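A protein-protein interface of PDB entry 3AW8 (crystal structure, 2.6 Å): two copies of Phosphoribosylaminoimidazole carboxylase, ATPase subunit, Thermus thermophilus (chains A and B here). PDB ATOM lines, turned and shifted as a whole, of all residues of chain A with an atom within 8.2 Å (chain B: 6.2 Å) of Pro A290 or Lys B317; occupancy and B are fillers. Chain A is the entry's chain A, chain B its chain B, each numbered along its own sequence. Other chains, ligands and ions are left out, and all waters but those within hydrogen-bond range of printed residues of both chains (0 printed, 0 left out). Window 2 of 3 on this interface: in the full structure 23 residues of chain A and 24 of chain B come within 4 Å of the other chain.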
ATOM      1  N   LEU A  21     -24.042 -17.977 -29.522  1.00  0.00           N
ATOM      2  CA  LEU A  21     -24.424 -18.265 -28.142  1.00  0.00           C
ATOM      3  C   LEU A  21     -25.445 -17.234 -27.677  1.00  0.00           C
ATOM      4  O   LEU A  21     -25.743 -17.134 -26.493  1.00  0.00           O
ATOM      5  CB  LEU A  21     -23.202 -18.232 -27.216  1.00  0.00           C
ATOM      6  CG  LEU A  21     -22.155 -19.335 -27.403  1.00  0.00           C
ATOM      7  CD1 LEU A  21     -20.946 -19.042 -26.561  1.00  0.00           C
ATOM      8  CD2 LEU A  21     -22.735 -20.678 -27.014  1.00  0.00           C
ATOM      9  N   VAL A 186      -6.827 -22.167 -21.149  1.00  0.00           N
ATOM     10  CA  VAL A 186      -8.010 -21.456 -20.708  1.00  0.00           C
ATOM     11  C   VAL A 186      -8.495 -21.926 -19.343  1.00  0.00           C
ATOM     12  O   VAL A 186      -8.441 -23.110 -19.014  1.00  0.00           O
ATOM     13  CB  VAL A 186      -9.139 -21.590 -21.760  1.00  0.00           C
ATOM     14  CG1 VAL A 186      -9.152 -22.991 -22.328  1.00  0.00           C
ATOM     15  CG2 VAL A 186     -10.485 -21.251 -21.138  1.00  0.00           C
ATOM     16  N   GLY A 188     -11.839 -21.288 -16.785  1.00  0.00           N
ATOM     17  CA  GLY A 188     -13.146 -20.701 -16.569  1.00  0.00           C
ATOM     18  C   GLY A 188     -13.276 -19.965 -15.246  1.00  0.00           C
ATOM     19  O   GLY A 188     -12.399 -20.026 -14.384  1.00  0.00           O
ATOM     20  N   ARG A 189     -14.386 -19.258 -15.091  1.00  0.00           N
ATOM     21  CA  ARG A 189     -14.650 -18.495 -13.884  1.00  0.00           C
ATOM     22  C   ARG A 189     -14.868 -19.477 -12.747  1.00  0.00           C
ATOM     23  O   ARG A 189     -14.655 -19.163 -11.574  1.00  0.00           O
ATOM     24  CB  ARG A 189     -15.895 -17.631 -14.089  1.00  0.00           C
ATOM     25  CG  ARG A 189     -16.071 -16.531 -13.069  1.00  0.00           C
ATOM     26  CD  ARG A 189     -17.118 -15.531 -13.530  1.00  0.00           C
ATOM     27  NE  ARG A 189     -18.447 -16.124 -13.632  1.00  0.00           N
ATOM     28  CZ  ARG A 189     -19.477 -15.552 -14.254  1.00  0.00           C
ATOM     29  NH1 ARG A 189     -19.335 -14.364 -14.840  1.00  0.00           N
ATOM     30  NH2 ARG A 189     -20.656 -16.167 -14.287  1.00  0.00           N
ATOM     31  N   THR A 190     -15.280 -20.683 -13.114  1.00  0.00           N
ATOM     32  CA  THR A 190     -15.553 -21.744 -12.157  1.00  0.00           C
ATOM     33  C   THR A 190     -14.286 -22.382 -11.599  1.00  0.00           C
ATOM     34  O   THR A 190     -14.299 -22.959 -10.514  1.00  0.00           O
ATOM     35  CB  THR A 190     -16.357 -22.846 -12.818  1.00  0.00           C
ATOM     36  OG1 THR A 190     -15.572 -23.418 -13.876  1.00  0.00           O
ATOM     37  CG2 THR A 190     -17.657 -22.285 -13.386  1.00  0.00           C
ATOM     38  N   GLU A 192     -12.473 -24.444 -13.704  1.00  0.00           N
ATOM     39  CA  GLU A 192     -12.171 -25.490 -14.680  1.00  0.00           C
ATOM     40  C   GLU A 192     -11.093 -24.984 -15.629  1.00  0.00           C
ATOM     41  O   GLU A 192     -10.950 -23.777 -15.817  1.00  0.00           O
ATOM     42  CB  GLU A 192     -13.428 -25.858 -15.473  1.00  0.00           C
ATOM     43  CG  GLU A 192     -13.174 -26.715 -16.711  1.00  0.00           C
ATOM     44  CD  GLU A 192     -14.451 -26.986 -17.490  1.00  0.00           C
ATOM     45  OE1 GLU A 192     -15.445 -26.260 -17.262  1.00  0.00           O
ATOM     46  OE2 GLU A 192     -14.464 -27.910 -18.334  1.00  0.00           O
ATOM     47  N   THR A 276     -13.449 -26.565 -30.427  1.00  0.00           N
ATOM     48  CA  THR A 276     -13.957 -25.319 -29.869  1.00  0.00           C
ATOM     49  C   THR A 276     -12.900 -24.269 -30.119  1.00  0.00           C
ATOM     50  O   THR A 276     -11.727 -24.473 -29.792  1.00  0.00           O
ATOM     51  CB  THR A 276     -14.183 -25.413 -28.341  1.00  0.00           C
ATOM     52  OG1 THR A 276     -14.937 -26.589 -28.029  1.00  0.00           O
ATOM     53  CG2 THR A 276     -14.953 -24.196 -27.847  1.00  0.00           C
ATOM     54  N   GLU A 280     -14.533 -18.876 -28.723  1.00  0.00           N
ATOM     55  CA  GLU A 280     -15.701 -19.360 -28.013  1.00  0.00           C
ATOM     56  C   GLU A 280     -15.325 -19.743 -26.576  1.00  0.00           C
ATOM     57  O   GLU A 280     -16.054 -19.436 -25.631  1.00  0.00           O
ATOM     58  CB  GLU A 280     -16.330 -20.561 -28.724  1.00  0.00           C
ATOM     59  CG  GLU A 280     -17.555 -21.085 -27.966  1.00  0.00           C
ATOM     60  CD  GLU A 280     -18.244 -22.269 -28.622  1.00  0.00           C
ATOM     61  OE1 GLU A 280     -18.956 -22.994 -27.894  1.00  0.00           O
ATOM     62  OE2 GLU A 280     -18.095 -22.471 -29.848  1.00  0.00           O
ATOM     63  N   ASN A 281     -14.183 -20.404 -26.406  1.00  0.00           N
ATOM     64  CA  ASN A 281     -13.751 -20.809 -25.072  1.00  0.00           C
ATOM     65  C   ASN A 281     -13.481 -19.629 -24.147  1.00  0.00           C
ATOM     66  O   ASN A 281     -13.799 -19.683 -22.951  1.00  0.00           O
ATOM     67  CB  ASN A 281     -12.511 -21.703 -25.161  1.00  0.00           C
ATOM     68  CG  ASN A 281     -12.820 -23.153 -24.833  1.00  0.00           C
ATOM     69  OD1 ASN A 281     -12.045 -24.054 -25.152  1.00  0.00           O
ATOM     70  ND2 ASN A 281     -13.955 -23.382 -24.184  1.00  0.00           N
ATOM     71  N   LEU A 283     -14.933 -16.855 -24.250  1.00  0.00           N
ATOM     72  CA  LEU A 283     -16.269 -16.397 -23.909  1.00  0.00           C
ATOM     73  C   LEU A 283     -16.900 -17.312 -22.862  1.00  0.00           C
ATOM     74  O   LEU A 283     -17.485 -16.838 -21.886  1.00  0.00           O
ATOM     75  CB  LEU A 283     -17.139 -16.352 -25.176  1.00  0.00           C
ATOM     76  CG  LEU A 283     -17.537 -15.008 -25.810  1.00  0.00           C
ATOM     77  CD1 LEU A 283     -16.517 -13.929 -25.520  1.00  0.00           C
ATOM     78  CD2 LEU A 283     -17.702 -15.213 -27.314  1.00  0.00           C
ATOM     79  N   ARG A 284     -16.779 -18.618 -23.064  1.00  0.00           N
ATOM     80  CA  ARG A 284     -17.350 -19.569 -22.120  1.00  0.00           C
ATOM     81  C   ARG A 284     -16.696 -19.396 -20.751  1.00  0.00           C
ATOM     82  O   ARG A 284     -17.378 -19.395 -19.721  1.00  0.00           O
ATOM     83  CB  ARG A 284     -17.188 -21.004 -22.649  1.00  0.00           C
ATOM     84  CG  ARG A 284     -18.118 -21.277 -23.827  1.00  0.00           C
ATOM     85  CD  ARG A 284     -17.717 -22.469 -24.693  1.00  0.00           C
ATOM     86  NE  ARG A 284     -18.150 -23.746 -24.135  1.00  0.00           N
ATOM     87  CZ  ARG A 284     -18.378 -24.844 -24.851  1.00  0.00           C
ATOM     88  NH1 ARG A 284     -18.226 -24.841 -26.170  1.00  0.00           N
ATOM     89  NH2 ARG A 284     -18.751 -25.956 -24.241  1.00  0.00           N
ATOM     90  N   ALA A 285     -15.380 -19.213 -20.753  1.00  0.00           N
ATOM     91  CA  ALA A 285     -14.636 -19.018 -19.519  1.00  0.00           C
ATOM     92  C   ALA A 285     -15.132 -17.811 -18.733  1.00  0.00           C
ATOM     93  O   ALA A 285     -15.634 -17.959 -17.622  1.00  0.00           O
ATOM     94  CB  ALA A 285     -13.162 -18.857 -19.816  1.00  0.00           C
ATOM     95  N   LEU A 287     -17.664 -16.276 -18.857  1.00  0.00           N
ATOM     96  CA  LEU A 287     -19.102 -16.313 -18.612  1.00  0.00           C
ATOM     97  C   LEU A 287     -19.476 -17.315 -17.528  1.00  0.00           C
ATOM     98  O   LEU A 287     -20.589 -17.291 -17.012  1.00  0.00           O
ATOM     99  CB  LEU A 287     -19.842 -16.636 -19.920  1.00  0.00           C
ATOM    100  CG  LEU A 287     -20.924 -15.658 -20.402  1.00  0.00           C
ATOM    101  CD1 LEU A 287     -20.605 -14.244 -19.973  1.00  0.00           C
ATOM    102  CD2 LEU A 287     -21.037 -15.750 -21.918  1.00  0.00           C
ATOM    103  N   GLY A 288     -18.536 -18.185 -17.174  1.00  0.00           N
ATOM    104  CA  GLY A 288     -18.798 -19.176 -16.148  1.00  0.00           C
ATOM    105  C   GLY A 288     -19.492 -20.400 -16.706  1.00  0.00           C
ATOM    106  O   GLY A 288     -20.102 -21.167 -15.970  1.00  0.00           O
ATOM    107  N   LEU A 289     -19.414 -20.581 -18.017  1.00  0.00           N
ATOM    108  CA  LEU A 289     -20.032 -21.733 -18.652  1.00  0.00           C
ATOM    109  C   LEU A 289     -18.999 -22.838 -18.784  1.00  0.00           C
ATOM    110  O   LEU A 289     -17.797 -22.587 -18.722  1.00  0.00           O
ATOM    111  CB  LEU A 289     -20.545 -21.358 -20.041  1.00  0.00           C
ATOM    112  CG  LEU A 289     -21.677 -20.340 -20.091  1.00  0.00           C
ATOM    113  CD1 LEU A 289     -21.809 -19.786 -21.502  1.00  0.00           C
ATOM    114  CD2 LEU A 289     -22.969 -20.995 -19.647  1.00  0.00           C
ATOM    115  N   PRO A 290     -19.456 -24.086 -18.944  1.00  0.00           N
ATOM    116  CA  PRO A 290     -18.537 -25.217 -19.093  1.00  0.00           C
ATOM    117  C   PRO A 290     -17.644 -24.971 -20.312  1.00  0.00           C
ATOM    118  O   PRO A 290     -18.121 -24.536 -21.355  1.00  0.00           O
ATOM    119  CB  PRO A 290     -19.480 -26.392 -19.308  1.00  0.00           C
ATOM    120  CG  PRO A 290     -20.693 -25.995 -18.508  1.00  0.00           C
ATOM    121  CD  PRO A 290     -20.853 -24.546 -18.863  1.00  0.00           C
ATOM    122  N   LEU A 291     -16.351 -25.227 -20.178  1.00  0.00           N
ATOM    123  CA  LEU A 291     -15.434 -25.027 -21.286  1.00  0.00           C
ATOM    124  C   LEU A 291     -15.671 -26.097 -22.334  1.00  0.00           C
ATOM    125  O   LEU A 291     -16.108 -27.198 -22.015  1.00  0.00           O
ATOM    126  CB  LEU A 291     -13.993 -25.091 -20.790  1.00  0.00           C
ATOM    127  CG  LEU A 291     -13.375 -23.781 -20.296  1.00  0.00           C
ATOM    128  CD1 LEU A 291     -14.418 -22.873 -19.670  1.00  0.00           C
ATOM    129  CD2 LEU A 291     -12.268 -24.116 -19.308  1.00  0.00           C
ATOM    130  N   GLY A 292     -15.393 -25.767 -23.587  1.00  0.00           N
ATOM    131  CA  GLY A 292     -15.590 -26.723 -24.655  1.00  0.00           C
ATOM    132  C   GLY A 292     -14.321 -27.498 -24.931  1.00  0.00           C
ATOM    133  O   GLY A 292     -13.218 -27.072 -24.574  1.00  0.00           O
ATOM    134  N   SER A 293     -14.484 -28.650 -25.568  1.00  0.00           N
ATOM    135  CA  SER A 293     -13.366 -29.510 -25.911  1.00  0.00           C
ATOM    136  C   SER A 293     -12.340 -28.777 -26.771  1.00  0.00           C
ATOM    137  O   SER A 293     -12.695 -27.991 -27.654  1.00  0.00           O
ATOM    138  CB  SER A 293     -13.876 -30.747 -26.654  1.00  0.00           C
ATOM    139  OG  SER A 293     -12.796 -31.554 -27.090  1.00  0.00           O
ATOM    140  N   PHE B 312     -28.279 -23.443 -20.950  1.00  0.00           N
ATOM    141  CA  PHE B 312     -27.002 -23.419 -21.658  1.00  0.00           C
ATOM    142  C   PHE B 312     -25.874 -24.200 -21.010  1.00  0.00           C
ATOM    143  O   PHE B 312     -25.148 -24.918 -21.694  1.00  0.00           O
ATOM    144  CB  PHE B 312     -26.566 -21.973 -21.915  1.00  0.00           C
ATOM    145  CG  PHE B 312     -27.373 -21.277 -22.978  1.00  0.00           C
ATOM    146  CD1 PHE B 312     -28.569 -21.822 -23.433  1.00  0.00           C
ATOM    147  CD2 PHE B 312     -26.956 -20.055 -23.498  1.00  0.00           C
ATOM    148  CE1 PHE B 312     -29.337 -21.167 -24.386  1.00  0.00           C
ATOM    149  CE2 PHE B 312     -27.722 -19.390 -24.452  1.00  0.00           C
ATOM    150  CZ  PHE B 312     -28.916 -19.948 -24.896  1.00  0.00           C
ATOM    151  N   ALA B 313     -25.720 -24.066 -19.701  1.00  0.00           N
ATOM    152  CA  ALA B 313     -24.667 -24.795 -19.004  1.00  0.00           C
ATOM    153  C   ALA B 313     -24.843 -26.290 -19.253  1.00  0.00           C
ATOM    154  O   ALA B 313     -23.872 -27.016 -19.454  1.00  0.00           O
ATOM    155  CB  ALA B 313     -24.724 -24.505 -17.521  1.00  0.00           C
ATOM    156  N   GLU B 314     -26.090 -26.742 -19.263  1.00  0.00           N
ATOM    157  CA  GLU B 314     -26.384 -28.153 -19.481  1.00  0.00           C
ATOM    158  C   GLU B 314     -26.036 -28.696 -20.864  1.00  0.00           C
ATOM    159  O   GLU B 314     -25.615 -29.844 -20.980  1.00  0.00           O
ATOM    160  CB  GLU B 314     -27.860 -28.432 -19.188  1.00  0.00           C
ATOM    161  CG  GLU B 314     -28.095 -29.474 -18.100  1.00  0.00           C
ATOM    162  CD  GLU B 314     -27.332 -29.167 -16.819  1.00  0.00           C
ATOM    163  OE1 GLU B 314     -26.176 -29.633 -16.675  1.00  0.00           O
ATOM    164  OE2 GLU B 314     -27.886 -28.444 -15.962  1.00  0.00           O
ATOM    165  N   VAL B 315     -26.210 -27.898 -21.916  1.00  0.00           N
ATOM    166  CA  VAL B 315     -25.892 -28.392 -23.250  1.00  0.00           C
ATOM    167  C   VAL B 315     -24.394 -28.288 -23.514  1.00  0.00           C
ATOM    168  O   VAL B 315     -23.812 -29.146 -24.178  1.00  0.00           O
ATOM    169  CB  VAL B 315     -26.688 -27.637 -24.366  1.00  0.00           C
ATOM    170  CG1 VAL B 315     -28.018 -27.155 -23.817  1.00  0.00           C
ATOM    171  CG2 VAL B 315     -25.874 -26.484 -24.937  1.00  0.00           C
ATOM    172  N   LEU B 316     -23.761 -27.247 -22.988  1.00  0.00           N
ATOM    173  CA  LEU B 316     -22.330 -27.084 -23.185  1.00  0.00           C
ATOM    174  C   LEU B 316     -21.541 -28.146 -22.408  1.00  0.00           C
ATOM    175  O   LEU B 316     -20.347 -28.327 -22.630  1.00  0.00           O
ATOM    176  CB  LEU B 316     -21.903 -25.675 -22.769  1.00  0.00           C
ATOM    177  CG  LEU B 316     -22.038 -24.507 -23.767  1.00  0.00           C
ATOM    178  CD1 LEU B 316     -22.908 -24.872 -24.948  1.00  0.00           C
ATOM    179  CD2 LEU B 316     -22.597 -23.293 -23.034  1.00  0.00           C
ATOM    180  N   LYS B 317     -22.217 -28.850 -21.498  1.00  0.00           N
ATOM    181  CA  LYS B 317     -21.590 -29.906 -20.704  1.00  0.00           C
ATOM    182  C   LYS B 317     -21.211 -31.079 -21.603  1.00  0.00           C
ATOM    183  O   LYS B 317     -20.233 -31.774 -21.339  1.00  0.00           O
ATOM    184  CB  LYS B 317     -22.548 -30.427 -19.623  1.00  0.00           C
ATOM    185  CG  LYS B 317     -22.741 -29.532 -18.412  1.00  0.00           C
ATOM    186  CD  LYS B 317     -21.463 -29.393 -17.599  1.00  0.00           C
ATOM    187  CE  LYS B 317     -21.666 -28.483 -16.383  1.00  0.00           C
ATOM    188  NZ  LYS B 317     -20.384 -28.213 -15.650  1.00  0.00           N
ATOM    189  N   VAL B 318     -21.996 -31.304 -22.656  1.00  0.00           N
ATOM    190  CA  VAL B 318     -21.733 -32.415 -23.566  1.00  0.00           C
ATOM    191  C   VAL B 318     -20.758 -32.070 -24.698  1.00  0.00           C
ATOM    192  O   VAL B 318     -20.910 -31.076 -25.409  1.00  0.00           O
ATOM    193  CB  VAL B 318     -23.072 -33.014 -24.118  1.00  0.00           C
ATOM    194  CG1 VAL B 318     -24.201 -32.059 -23.875  1.00  0.00           C
ATOM    195  CG2 VAL B 318     -22.950 -33.363 -25.590  1.00  0.00           C
ATOM    196  N   GLU B 319     -19.739 -32.910 -24.833  1.00  0.00           N
ATOM    197  CA  GLU B 319     -18.699 -32.721 -25.829  1.00  0.00           C
ATOM    198  C   GLU B 319     -19.230 -32.915 -27.234  1.00  0.00           C
ATOM    199  O   GLU B 319     -20.087 -33.768 -27.477  1.00  0.00           O
ATOM    200  CB  GLU B 319     -17.542 -33.692 -25.555  1.00  0.00           C
ATOM    201  CG  GLU B 319     -16.404 -33.648 -26.572  1.00  0.00           C
ATOM    202  CD  GLU B 319     -15.225 -34.525 -26.163  1.00  0.00           C
ATOM    203  OE1 GLU B 319     -14.319 -34.745 -27.001  1.00  0.00           O
ATOM    204  OE2 GLU B 319     -15.207 -34.986 -24.997  1.00  0.00           O
ATOM    205  N   ARG B 355     -28.004 -37.704 -24.133  1.00  0.00           N
ATOM    206  CA  ARG B 355     -27.901 -36.725 -23.061  1.00  0.00           C
ATOM    207  C   ARG B 355     -28.601 -35.409 -23.386  1.00  0.00           C
ATOM    208  O   ARG B 355     -29.121 -34.738 -22.490  1.00  0.00           O
ATOM    209  CB  ARG B 355     -26.439 -36.452 -22.707  1.00  0.00           C
ATOM    210  CG  ARG B 355     -26.203 -36.470 -21.206  1.00  0.00           C
ATOM    211  CD  ARG B 355     -25.055 -35.576 -20.774  1.00  0.00           C
ATOM    212  NE  ARG B 355     -23.815 -35.857 -21.490  1.00  0.00           N
ATOM    213  CZ  ARG B 355     -22.655 -35.261 -21.222  1.00  0.00           C
ATOM    214  NH1 ARG B 355     -22.584 -34.357 -20.246  1.00  0.00           N
ATOM    215  NH2 ARG B 355     -21.574 -35.555 -21.944  1.00  0.00           N
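The guanidinium group (NH2) of Arg A284 sits at hydrogen-bond distance from the backbone carbonyl oxygen (O) of Leu B316.
Lys B317 touches just one residue of chain A: Pro A290.
Of the printed residues of chain B, Arg A284 touches Leu B316 (3.3 Å).
Printed residues of chain B within 4 Å of Leu A21: Phe B312 (3.6 Å).
Leu A287 touches none of the printed residues of chain B.
Leu A291 touches none of the printed residues of chain B.
The nearest printed residue of chain B that does not touch Leu A21 is Leu B316 (4.7 Å).
Among the printed residues, merely in contact across the chains: Leu A21 with Phe B312, Leu A289 with Leu B316, Pro A290 with Ala B313, Pro A290 with Leu B316, Pro A290 with Lys B317 and Ser A293 with Glu B319.
No position is printed for both chains.
The side-chain hydroxyl (OG1) of Thr A276 lies within hydrogen-bond range of the backbone carbonyl oxygen (O) of Ser A293, at 2.7 Å.
The guanidinium group (NH1) of Arg A284 lies within salt-bridge range of the side-chain carboxylate (OE1) of Glu A280.
O of Arg A284 sits at hydrogen-bond distance from N of Leu A289, at 2.9 Å.
The backbone carbonyl oxygen (O) of Pro A290 sits at hydrogen-bond distance from the guanidinium group (NE) of Arg A284.
Hydrophobic or aromatic side chains of chain A within 4 Å of the printed part of chain B: Leu A289 and Pro A290.
Along chain A the printed residues that touch a printed residue of chain B span positions 21 to 293.
Among the printed residues, 7 pairs touch across the chains.
Among the printed residues, no Asp or Glu carboxylate lies within 4 Å of a Lys or Arg side-chain nitrogen of the other chain.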
